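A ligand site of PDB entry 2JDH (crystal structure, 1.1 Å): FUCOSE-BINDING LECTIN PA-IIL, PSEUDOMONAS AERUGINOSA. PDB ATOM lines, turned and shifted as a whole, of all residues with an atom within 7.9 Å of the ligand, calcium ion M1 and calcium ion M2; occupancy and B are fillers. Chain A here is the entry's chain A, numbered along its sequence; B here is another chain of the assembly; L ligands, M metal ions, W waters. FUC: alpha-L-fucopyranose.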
ATOM      1  N   ALA A  21       9.285  -0.289 -30.901  1.00  0.00           N
ATOM      2  CA  ALA A  21       9.473   0.706 -29.820  1.00  0.00           C
ATOM      3  C   ALA A  21       9.697   0.030 -28.475  1.00  0.00           C
ATOM      4  O   ALA A  21       9.069  -1.009 -28.149  1.00  0.00           O
ATOM      5  CB  ALA A  21       8.228   1.602 -29.737  1.00  0.00           C
ATOM      6  N   ASN A  22      10.626   0.634 -27.695  1.00  0.00           N
ATOM      7  CA  ASN A  22      10.939   0.137 -26.347  1.00  0.00           C
ATOM      8  C   ASN A  22      11.272   1.317 -25.454  1.00  0.00           C
ATOM      9  O   ASN A  22      12.450   1.547 -25.118  1.00  0.00           O
ATOM     10  CB  ASN A  22      12.154  -0.796 -26.354  1.00  0.00           C
ATOM     11  CG  ASN A  22      11.824  -2.127 -27.020  1.00  0.00           C
ATOM     12  OD1 ASN A  22      11.187  -3.020 -26.424  1.00  0.00           O
ATOM     13  ND2 ASN A  22      12.236  -2.286 -28.275  1.00  0.00           N
ATOM     14  N   SER A  23      10.244   2.115 -25.089  1.00  0.00           N
ATOM     15  CA  SER A  23      10.530   3.344 -24.336  1.00  0.00           C
ATOM     16  C   SER A  23       9.195   3.861 -23.800  1.00  0.00           C
ATOM     17  O   SER A  23       8.118   3.621 -24.356  1.00  0.00           O
ATOM     18  CB  SER A  23      11.113   4.413 -25.305  1.00  0.00           C
ATOM     19  OG  SER A  23      11.216   5.669 -24.610  1.00  0.00           O
ATOM     20  N   SER A  24       9.292   4.647 -22.707  1.00  0.00           N
ATOM     21  CA  SER A  24       8.112   5.397 -22.276  1.00  0.00           C
ATOM     22  C   SER A  24       7.646   6.411 -23.283  1.00  0.00           C
ATOM     23  O   SER A  24       6.437   6.748 -23.283  1.00  0.00           O
ATOM     24  CB  SER A  24       8.453   6.136 -20.949  1.00  0.00           C
ATOM     25  OG  SER A  24       9.432   7.178 -21.230  1.00  0.00           O
ATOM     26  N   GLY A  25       8.551   6.914 -24.128  1.00  0.00           N
ATOM     27  CA  GLY A  25       8.192   8.008 -25.003  1.00  0.00           C
ATOM     28  C   GLY A  25       7.714   7.563 -26.358  1.00  0.00           C
ATOM     29  O   GLY A  25       8.101   6.511 -26.886  1.00  0.00           O
ATOM     30  N   GLN A  27       7.736   7.315 -30.136  1.00  0.00           N
ATOM     31  CA  GLN A  27       8.769   7.413 -31.168  1.00  0.00           C
ATOM     32  C   GLN A  27       8.165   7.843 -32.470  1.00  0.00           C
ATOM     33  O   GLN A  27       7.116   7.301 -32.866  1.00  0.00           O
ATOM     34  CB  GLN A  27       9.408   6.007 -31.383  1.00  0.00           C
ATOM     35  CG  GLN A  27       9.792   5.305 -30.062  1.00  0.00           C
ATOM     36  CD  GLN A  27      10.983   5.965 -29.408  1.00  0.00           C
ATOM     37  OE1 GLN A  27      12.031   6.126 -30.015  1.00  0.00           O
ATOM     38  NE2 GLN A  27      10.846   6.307 -28.107  1.00  0.00           N
ATOM     39  N   GLN A  44       4.059   4.098 -29.342  1.00  0.00           N
ATOM     40  CA  GLN A  44       4.678   3.977 -28.028  1.00  0.00           C
ATOM     41  C   GLN A  44       4.501   2.562 -27.515  1.00  0.00           C
ATOM     42  O   GLN A  44       3.366   2.029 -27.529  1.00  0.00           O
ATOM     43  CB  GLN A  44       4.038   4.973 -27.050  1.00  0.00           C
ATOM     44  CG  GLN A  44       4.729   5.068 -25.678  1.00  0.00           C
ATOM     45  CD  GLN A  44       4.320   3.955 -24.740  1.00  0.00           C
ATOM     46  OE1 GLN A  44       3.115   3.630 -24.646  1.00  0.00           O
ATOM     47  NE2 GLN A  44       5.244   3.351 -23.993  1.00  0.00           N
ATOM     48  N   SER A  45       5.598   1.981 -27.032  1.00  0.00           N
ATOM     49  CA  SER A  45       5.567   0.650 -26.418  1.00  0.00           C
ATOM     50  C   SER A  45       6.786   0.481 -25.584  1.00  0.00           C
ATOM     51  O   SER A  45       7.851   0.964 -25.967  1.00  0.00           O
ATOM     52  CB  SER A  45       5.565  -0.430 -27.545  1.00  0.00           C
ATOM     53  OG  SER A  45       5.546  -1.736 -26.995  1.00  0.00           O
ATOM     54  N   THR A  46       6.652  -0.272 -24.465  1.00  0.00           N
ATOM     55  CA  THR A  46       7.804  -0.759 -23.743  1.00  0.00           C
ATOM     56  C   THR A  46       7.950  -2.260 -23.951  1.00  0.00           C
ATOM     57  O   THR A  46       8.709  -2.909 -23.220  1.00  0.00           O
ATOM     58  CB  THR A  46       7.761  -0.403 -22.241  1.00  0.00           C
ATOM     59  OG1 THR A  46       6.472  -0.768 -21.747  1.00  0.00           O
ATOM     60  CG2 THR A  46       8.037   1.057 -22.051  1.00  0.00           C
ATOM     61  N   VAL A  70      11.949  11.884 -30.526  1.00  0.00           N
ATOM     62  CA  VAL A  70      11.126  11.577 -29.367  1.00  0.00           C
ATOM     63  C   VAL A  70      11.061  12.856 -28.526  1.00  0.00           C
ATOM     64  O   VAL A  70      12.102  13.497 -28.277  1.00  0.00           O
ATOM     65  CB  VAL A  70      11.786  10.476 -28.495  1.00  0.00           C
ATOM     66  CG1 VAL A  70      10.837  10.102 -27.297  1.00  0.00           C
ATOM     67  CG2 VAL A  70      12.050   9.226 -29.348  1.00  0.00           C
ATOM     68  N   SER A  95      18.433   3.389 -31.441  1.00  0.00           N
ATOM     69  CA  SER A  95      18.370   4.819 -31.089  1.00  0.00           C
ATOM     70  C   SER A  95      18.129   4.976 -29.599  1.00  0.00           C
ATOM     71  O   SER A  95      17.494   4.121 -28.968  1.00  0.00           O
ATOM     72  CB  SER A  95      17.257   5.510 -31.903  1.00  0.00           C
ATOM     73  OG  SER A  95      15.955   4.980 -31.567  1.00  0.00           O
ATOM     74  N   GLU A  96      18.642   6.100 -29.080  1.00  0.00           N
ATOM     75  CA  GLU A  96      18.572   6.396 -27.649  1.00  0.00           C
ATOM     76  C   GLU A  96      17.912   7.760 -27.469  1.00  0.00           C
ATOM     77  O   GLU A  96      18.411   8.760 -27.962  1.00  0.00           O
ATOM     78  CB  GLU A  96      19.974   6.375 -27.027  1.00  0.00           C
ATOM     79  CG  GLU A  96      19.990   6.744 -25.536  1.00  0.00           C
ATOM     80  CD  GLU A  96      19.061   5.842 -24.730  1.00  0.00           C
ATOM     81  OE1 GLU A  96      19.096   4.583 -24.886  1.00  0.00           O
ATOM     82  OE2 GLU A  96      18.218   6.357 -23.953  1.00  0.00           O
ATOM     83  N   ASP A  97      16.810   7.746 -26.714  1.00  0.00           N
ATOM     84  CA  ASP A  97      16.024   8.963 -26.472  1.00  0.00           C
ATOM     85  C   ASP A  97      16.270   9.551 -25.092  1.00  0.00           C
ATOM     86  O   ASP A  97      15.690  10.614 -24.772  1.00  0.00           O
ATOM     87  CB  ASP A  97      14.522   8.680 -26.683  1.00  0.00           C
ATOM     88  CG  ASP A  97      13.886   7.737 -25.684  1.00  0.00           C
ATOM     89  OD1 ASP A  97      14.387   7.624 -24.525  1.00  0.00           O
ATOM     90  OD2 ASP A  97      12.856   7.124 -26.039  1.00  0.00           O
ATOM     91  N   GLY A  98      17.091   8.911 -24.271  1.00  0.00           N
ATOM     92  CA  GLY A  98      17.221   9.227 -22.840  1.00  0.00           C
ATOM     93  C   GLY A  98      18.647   9.063 -22.367  1.00  0.00           C
ATOM     94  O   GLY A  98      19.615   9.451 -23.051  1.00  0.00           O
ATOM     95  N   THR A  99      18.765   8.503 -21.164  1.00  0.00           N
ATOM     96  CA  THR A  99      20.041   8.502 -20.476  1.00  0.00           C
ATOM     97  C   THR A  99      20.541   7.079 -20.184  1.00  0.00           C
ATOM     98  O   THR A  99      21.700   6.947 -19.731  1.00  0.00           O
ATOM     99  CB  THR A  99      19.943   9.267 -19.140  1.00  0.00           C
ATOM    100  OG1 THR A  99      18.932   8.691 -18.316  1.00  0.00           O
ATOM    101  CG2 THR A  99      19.575  10.737 -19.417  1.00  0.00           C
ATOM    102  N   ASP A 100      19.742   6.020 -20.364  1.00  0.00           N
ATOM    103  CA  ASP A 100      20.152   4.715 -19.970  1.00  0.00           C
ATOM    104  C   ASP A 100      21.027   4.012 -20.991  1.00  0.00           C
ATOM    105  O   ASP A 100      21.629   2.964 -20.675  1.00  0.00           O
ATOM    106  CB  ASP A 100      18.996   3.819 -19.544  1.00  0.00           C
ATOM    107  CG  ASP A 100      18.059   3.454 -20.705  1.00  0.00           C
ATOM    108  OD1 ASP A 100      18.168   4.105 -21.768  1.00  0.00           O
ATOM    109  OD2 ASP A 100      17.216   2.563 -20.487  1.00  0.00           O
ATOM    110  N   ASN A 101      21.100   4.547 -22.197  1.00  0.00           N
ATOM    111  CA  ASN A 101      21.987   3.958 -23.245  1.00  0.00           C
ATOM    112  C   ASN A 101      21.664   2.508 -23.559  1.00  0.00           C
ATOM    113  O   ASN A 101      22.594   1.735 -23.869  1.00  0.00           O
ATOM    114  CB  ASN A 101      23.441   4.198 -22.896  1.00  0.00           C
ATOM    115  CG  ASN A 101      23.748   5.678 -22.891  1.00  0.00           C
ATOM    116  OD1 ASN A 101      23.067   6.471 -23.563  1.00  0.00           O
ATOM    117  ND2 ASN A 101      24.776   6.092 -22.151  1.00  0.00           N
ATOM    118  N   ASP A 102      20.375   2.136 -23.561  1.00  0.00           N
ATOM    119  CA  ASP A 102      20.033   0.827 -24.069  1.00  0.00           C
ATOM    120  C   ASP A 102      19.892   0.827 -25.600  1.00  0.00           C
ATOM    121  O   ASP A 102      19.943  -0.249 -26.199  1.00  0.00           O
ATOM    122  CB  ASP A 102      18.789   0.181 -23.379  1.00  0.00           C
ATOM    123  CG  ASP A 102      17.450   0.979 -23.494  1.00  0.00           C
ATOM    124  OD1 ASP A 102      17.478   2.075 -24.132  1.00  0.00           O
ATOM    125  OD2 ASP A 102      16.447   0.423 -23.017  1.00  0.00           O
ATOM    126  N   TYR A 103      19.728   1.991 -26.221  1.00  0.00           N
ATOM    127  CA  TYR A 103      19.703   2.114 -27.688  1.00  0.00           C
ATOM    128  C   TYR A 103      18.620   1.307 -28.378  1.00  0.00           C
ATOM    129  O   TYR A 103      18.712   1.032 -29.588  1.00  0.00           O
ATOM    130  CB  TYR A 103      21.134   1.901 -28.301  1.00  0.00           C
ATOM    131  CG  TYR A 103      21.946   3.193 -28.188  1.00  0.00           C
ATOM    132  CD1 TYR A 103      21.914   4.164 -29.181  1.00  0.00           C
ATOM    133  CD2 TYR A 103      22.638   3.420 -27.038  1.00  0.00           C
ATOM    134  CE1 TYR A 103      22.595   5.363 -29.045  1.00  0.00           C
ATOM    135  CE2 TYR A 103      23.297   4.633 -26.844  1.00  0.00           C
ATOM    136  CZ  TYR A 103      23.245   5.558 -27.831  1.00  0.00           C
ATOM    137  OH  TYR A 103      23.920   6.786 -27.639  1.00  0.00           O
ATOM    138  N   ASN A 104      17.561   0.956 -27.640  1.00  0.00           N
ATOM    139  CA  ASN A 104      16.492   0.146 -28.248  1.00  0.00           C
ATOM    140  C   ASN A 104      15.189   0.927 -28.330  1.00  0.00           C
ATOM    141  O   ASN A 104      14.124   0.380 -28.604  1.00  0.00           O
ATOM    142  CB  ASN A 104      16.249  -1.143 -27.431  1.00  0.00           C
ATOM    143  CG  ASN A 104      15.622  -0.858 -26.089  1.00  0.00           C
ATOM    144  OD1 ASN A 104      15.376   0.314 -25.750  1.00  0.00           O
ATOM    145  ND2 ASN A 104      15.335  -1.893 -25.313  1.00  0.00           N
ATOM    146  N   ASP A 105      15.251   2.259 -28.072  1.00  0.00           N
ATOM    147  CA  ASP A 105      14.007   3.006 -27.814  1.00  0.00           C
ATOM    148  C   ASP A 105      13.137   3.017 -29.084  1.00  0.00           C
ATOM    149  O   ASP A 105      11.910   2.861 -29.008  1.00  0.00           O
ATOM    150  CB  ASP A 105      14.376   4.410 -27.340  1.00  0.00           C
ATOM    151  CG  ASP A 105      15.143   4.355 -26.044  1.00  0.00           C
ATOM    152  OD1 ASP A 105      14.874   3.464 -25.180  1.00  0.00           O
ATOM    153  OD2 ASP A 105      16.046   5.215 -25.842  1.00  0.00           O
ATOM    154  N   ALA A 106      13.791   3.220 -30.230  1.00  0.00           N
ATOM    155  CA  ALA A 106      13.208   2.787 -31.537  1.00  0.00           C
ATOM    156  C   ALA A 106      14.284   1.935 -32.177  1.00  0.00           C
ATOM    157  O   ALA A 106      15.472   2.370 -32.278  1.00  0.00           O
ATOM    158  CB  ALA A 106      12.856   3.932 -32.431  1.00  0.00           C
ATOM    159  N   PRO B 113      18.331  -6.007 -25.785  1.00  0.00           N
ATOM    160  CA  PRO B 113      17.243  -6.097 -24.805  1.00  0.00           C
ATOM    161  C   PRO B 113      16.031  -5.302 -25.273  1.00  0.00           C
ATOM    162  O   PRO B 113      16.088  -4.473 -26.182  1.00  0.00           O
ATOM    163  CB  PRO B 113      17.859  -5.431 -23.534  1.00  0.00           C
ATOM    164  CG  PRO B 113      18.775  -4.377 -24.151  1.00  0.00           C
ATOM    165  CD  PRO B 113      19.395  -5.075 -25.389  1.00  0.00           C
ATOM    166  N   LEU B 114      14.940  -5.570 -24.549  1.00  0.00           N
ATOM    167  CA  LEU B 114      13.663  -4.865 -24.760  1.00  0.00           C
ATOM    168  C   LEU B 114      13.459  -3.902 -23.578  1.00  0.00           C
ATOM    169  O   LEU B 114      14.241  -3.839 -22.614  1.00  0.00           O
ATOM    170  CB  LEU B 114      12.512  -5.865 -24.793  1.00  0.00           C
ATOM    171  CG  LEU B 114      12.652  -6.972 -25.852  1.00  0.00           C
ATOM    172  CD1 LEU B 114      11.339  -7.743 -25.892  1.00  0.00           C
ATOM    173  CD2 LEU B 114      13.030  -6.400 -27.252  1.00  0.00           C
ATOM    174  N   GLY B 115      12.351  -3.156 -23.672  1.00  0.00           N
ATOM    175  CA  GLY B 115      11.940  -2.279 -22.571  1.00  0.00           C
ATOM    176  C   GLY B 115      12.512  -0.909 -22.565  1.00  0.00           C
ATOM    177  O   GLY B 115      13.527  -0.618 -23.212  1.00  0.00           O
ATOM    178  OXT GLY B 115      11.920  -0.079 -21.783  1.00  0.00           O
HETATM  179  C1  FUC L   1      12.849   5.734 -21.680  1.00  0.00           C
HETATM  180  C2  FUC L   1      13.962   4.934 -22.387  1.00  0.00           C
HETATM  181  C3  FUC L   1      14.464   3.850 -21.481  1.00  0.00           C
HETATM  182  C4  FUC L   1      13.339   2.955 -21.033  1.00  0.00           C
HETATM  183  C5  FUC L   1      12.229   3.777 -20.390  1.00  0.00           C
HETATM  184  C6  FUC L   1      10.999   2.921 -20.051  1.00  0.00           C
HETATM  185  O1  FUC L   1      13.450   6.365 -20.535  1.00  0.00           O
HETATM  186  O2  FUC L   1      15.043   5.762 -22.795  1.00  0.00           O
HETATM  187  O3  FUC L   1      15.420   3.052 -22.252  1.00  0.00           O
HETATM  188  O4  FUC L   1      12.875   2.228 -22.212  1.00  0.00           O
HETATM  189  O5  FUC L   1      11.817   4.834 -21.281  1.00  0.00           O
HETATM  190 CA    CA M   1      14.480   1.504 -23.946  1.00  0.00          CA
HETATM  191 CA    CA M   2      16.927   4.336 -23.746  1.00  0.00          CA
HETATM  192  O   HOH W   1      16.577   6.782 -20.390  1.00  0.00           O
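Of the 25 residues printed, 4 come within 4 Å of calcium ion M2.
Along chain A the residues within 4 Å of calcium ion M2 span positions 96 to 105.
The nearest printed residue that does not touch calcium ion M2 is Asp 97 (4.2 Å).
Calcium ion M1 is bound by the side-chain amide oxygen (OD1) of Asn 104 (2.3 Å), the backbone carbonyl oxygen (O) of Asn 22 (2.3 Å), the side-chain carboxylate (OD1) of Asp 105 (2.3 Å), the side-chain carboxylate (OD2) of Asp 102 (2.4 Å), the chain-end carboxylate (O) of Gly 115 of chain B (2.4 Å), an oxygen (O4) of the ligand (2.5 Å) and an oxygen (O3) of the ligand (2.5 Å).
Slightly farther from calcium ion M1 lies OD1 of Asp 102 (3.1 Å).
O of Ser 95 lies within hydrogen-bond range of N of Asn 104, 3.4 Å away.
The side-chain amide nitrogen of Gln 44 is in hydrogen-bond range of the backbone carbonyl oxygen of Ser 23 (2.9 Å).
OE2 of Glu 96 sits close to N of Gly 98 (2.8 Å).
The side-chain amide nitrogen (ND2) of Asn 104 lies within hydrogen-bond range of the backbone carbonyl oxygen (O) of Pro 113 of chain B, 2.8 Å away.
O of Asp 105 lies close to OE1 of Gln 27 (3.4 Å).
The side-chain amide nitrogen of Gln 27 is in hydrogen-bond range of the side-chain carboxylate of Asp 97.
The side-chain carboxylate (OE1) of Glu 96 sits close to the backbone NH (N) of Asn 101 (3.4 Å).
The backbone NH of Ser 23 lies within hydrogen-bond range of the backbone carbonyl oxygen of Ser 45 (2.8 Å).
Within 4 Å of calcium ion M1: Asn 22, Asp 102, Asn 104, Asp 105 and Gly 115 of chain B.
The nearest printed residue that does not touch calcium ion M1 is Ser 23 (4.4 Å).
Of the 25 residues printed, 9 come within 4 Å of the ligand.
Calcium ion M2 is bound by the side-chain carboxylate (OD1) of Asp 100, the side-chain carboxylate (OD1) of Asp 102, the side-chain carboxylate (OE2) of Glu 96, the side-chain carboxylate (OD2) of Asp 105, the side-chain carboxylate (OE1) of Glu 96, an oxygen (O3) of the ligand, an oxygen (O2) of the ligand and the side-chain carboxylate (OD1) of Asp 105.
Water W1 lies within hydrogen-bond range of N of Thr 99 (2.9 Å), O1 of the ligand (3.2 Å) and N of Asp 100 (3.3 Å).
OG of Ser 24 is in hydrogen-bond range of O5 of the ligand, at 3.3 Å.
The backbone NH (N) of Ser 24 sits at hydrogen-bond distance from an oxygen (O5) of the ligand, 2.9 Å away.
The side-chain hydroxyl of Ser 23 lies close to an oxygen (O5) of the ligand.
The side-chain carboxylate of Asp 97 lies close to an oxygen (O2) of the ligand, at 2.6 Å.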
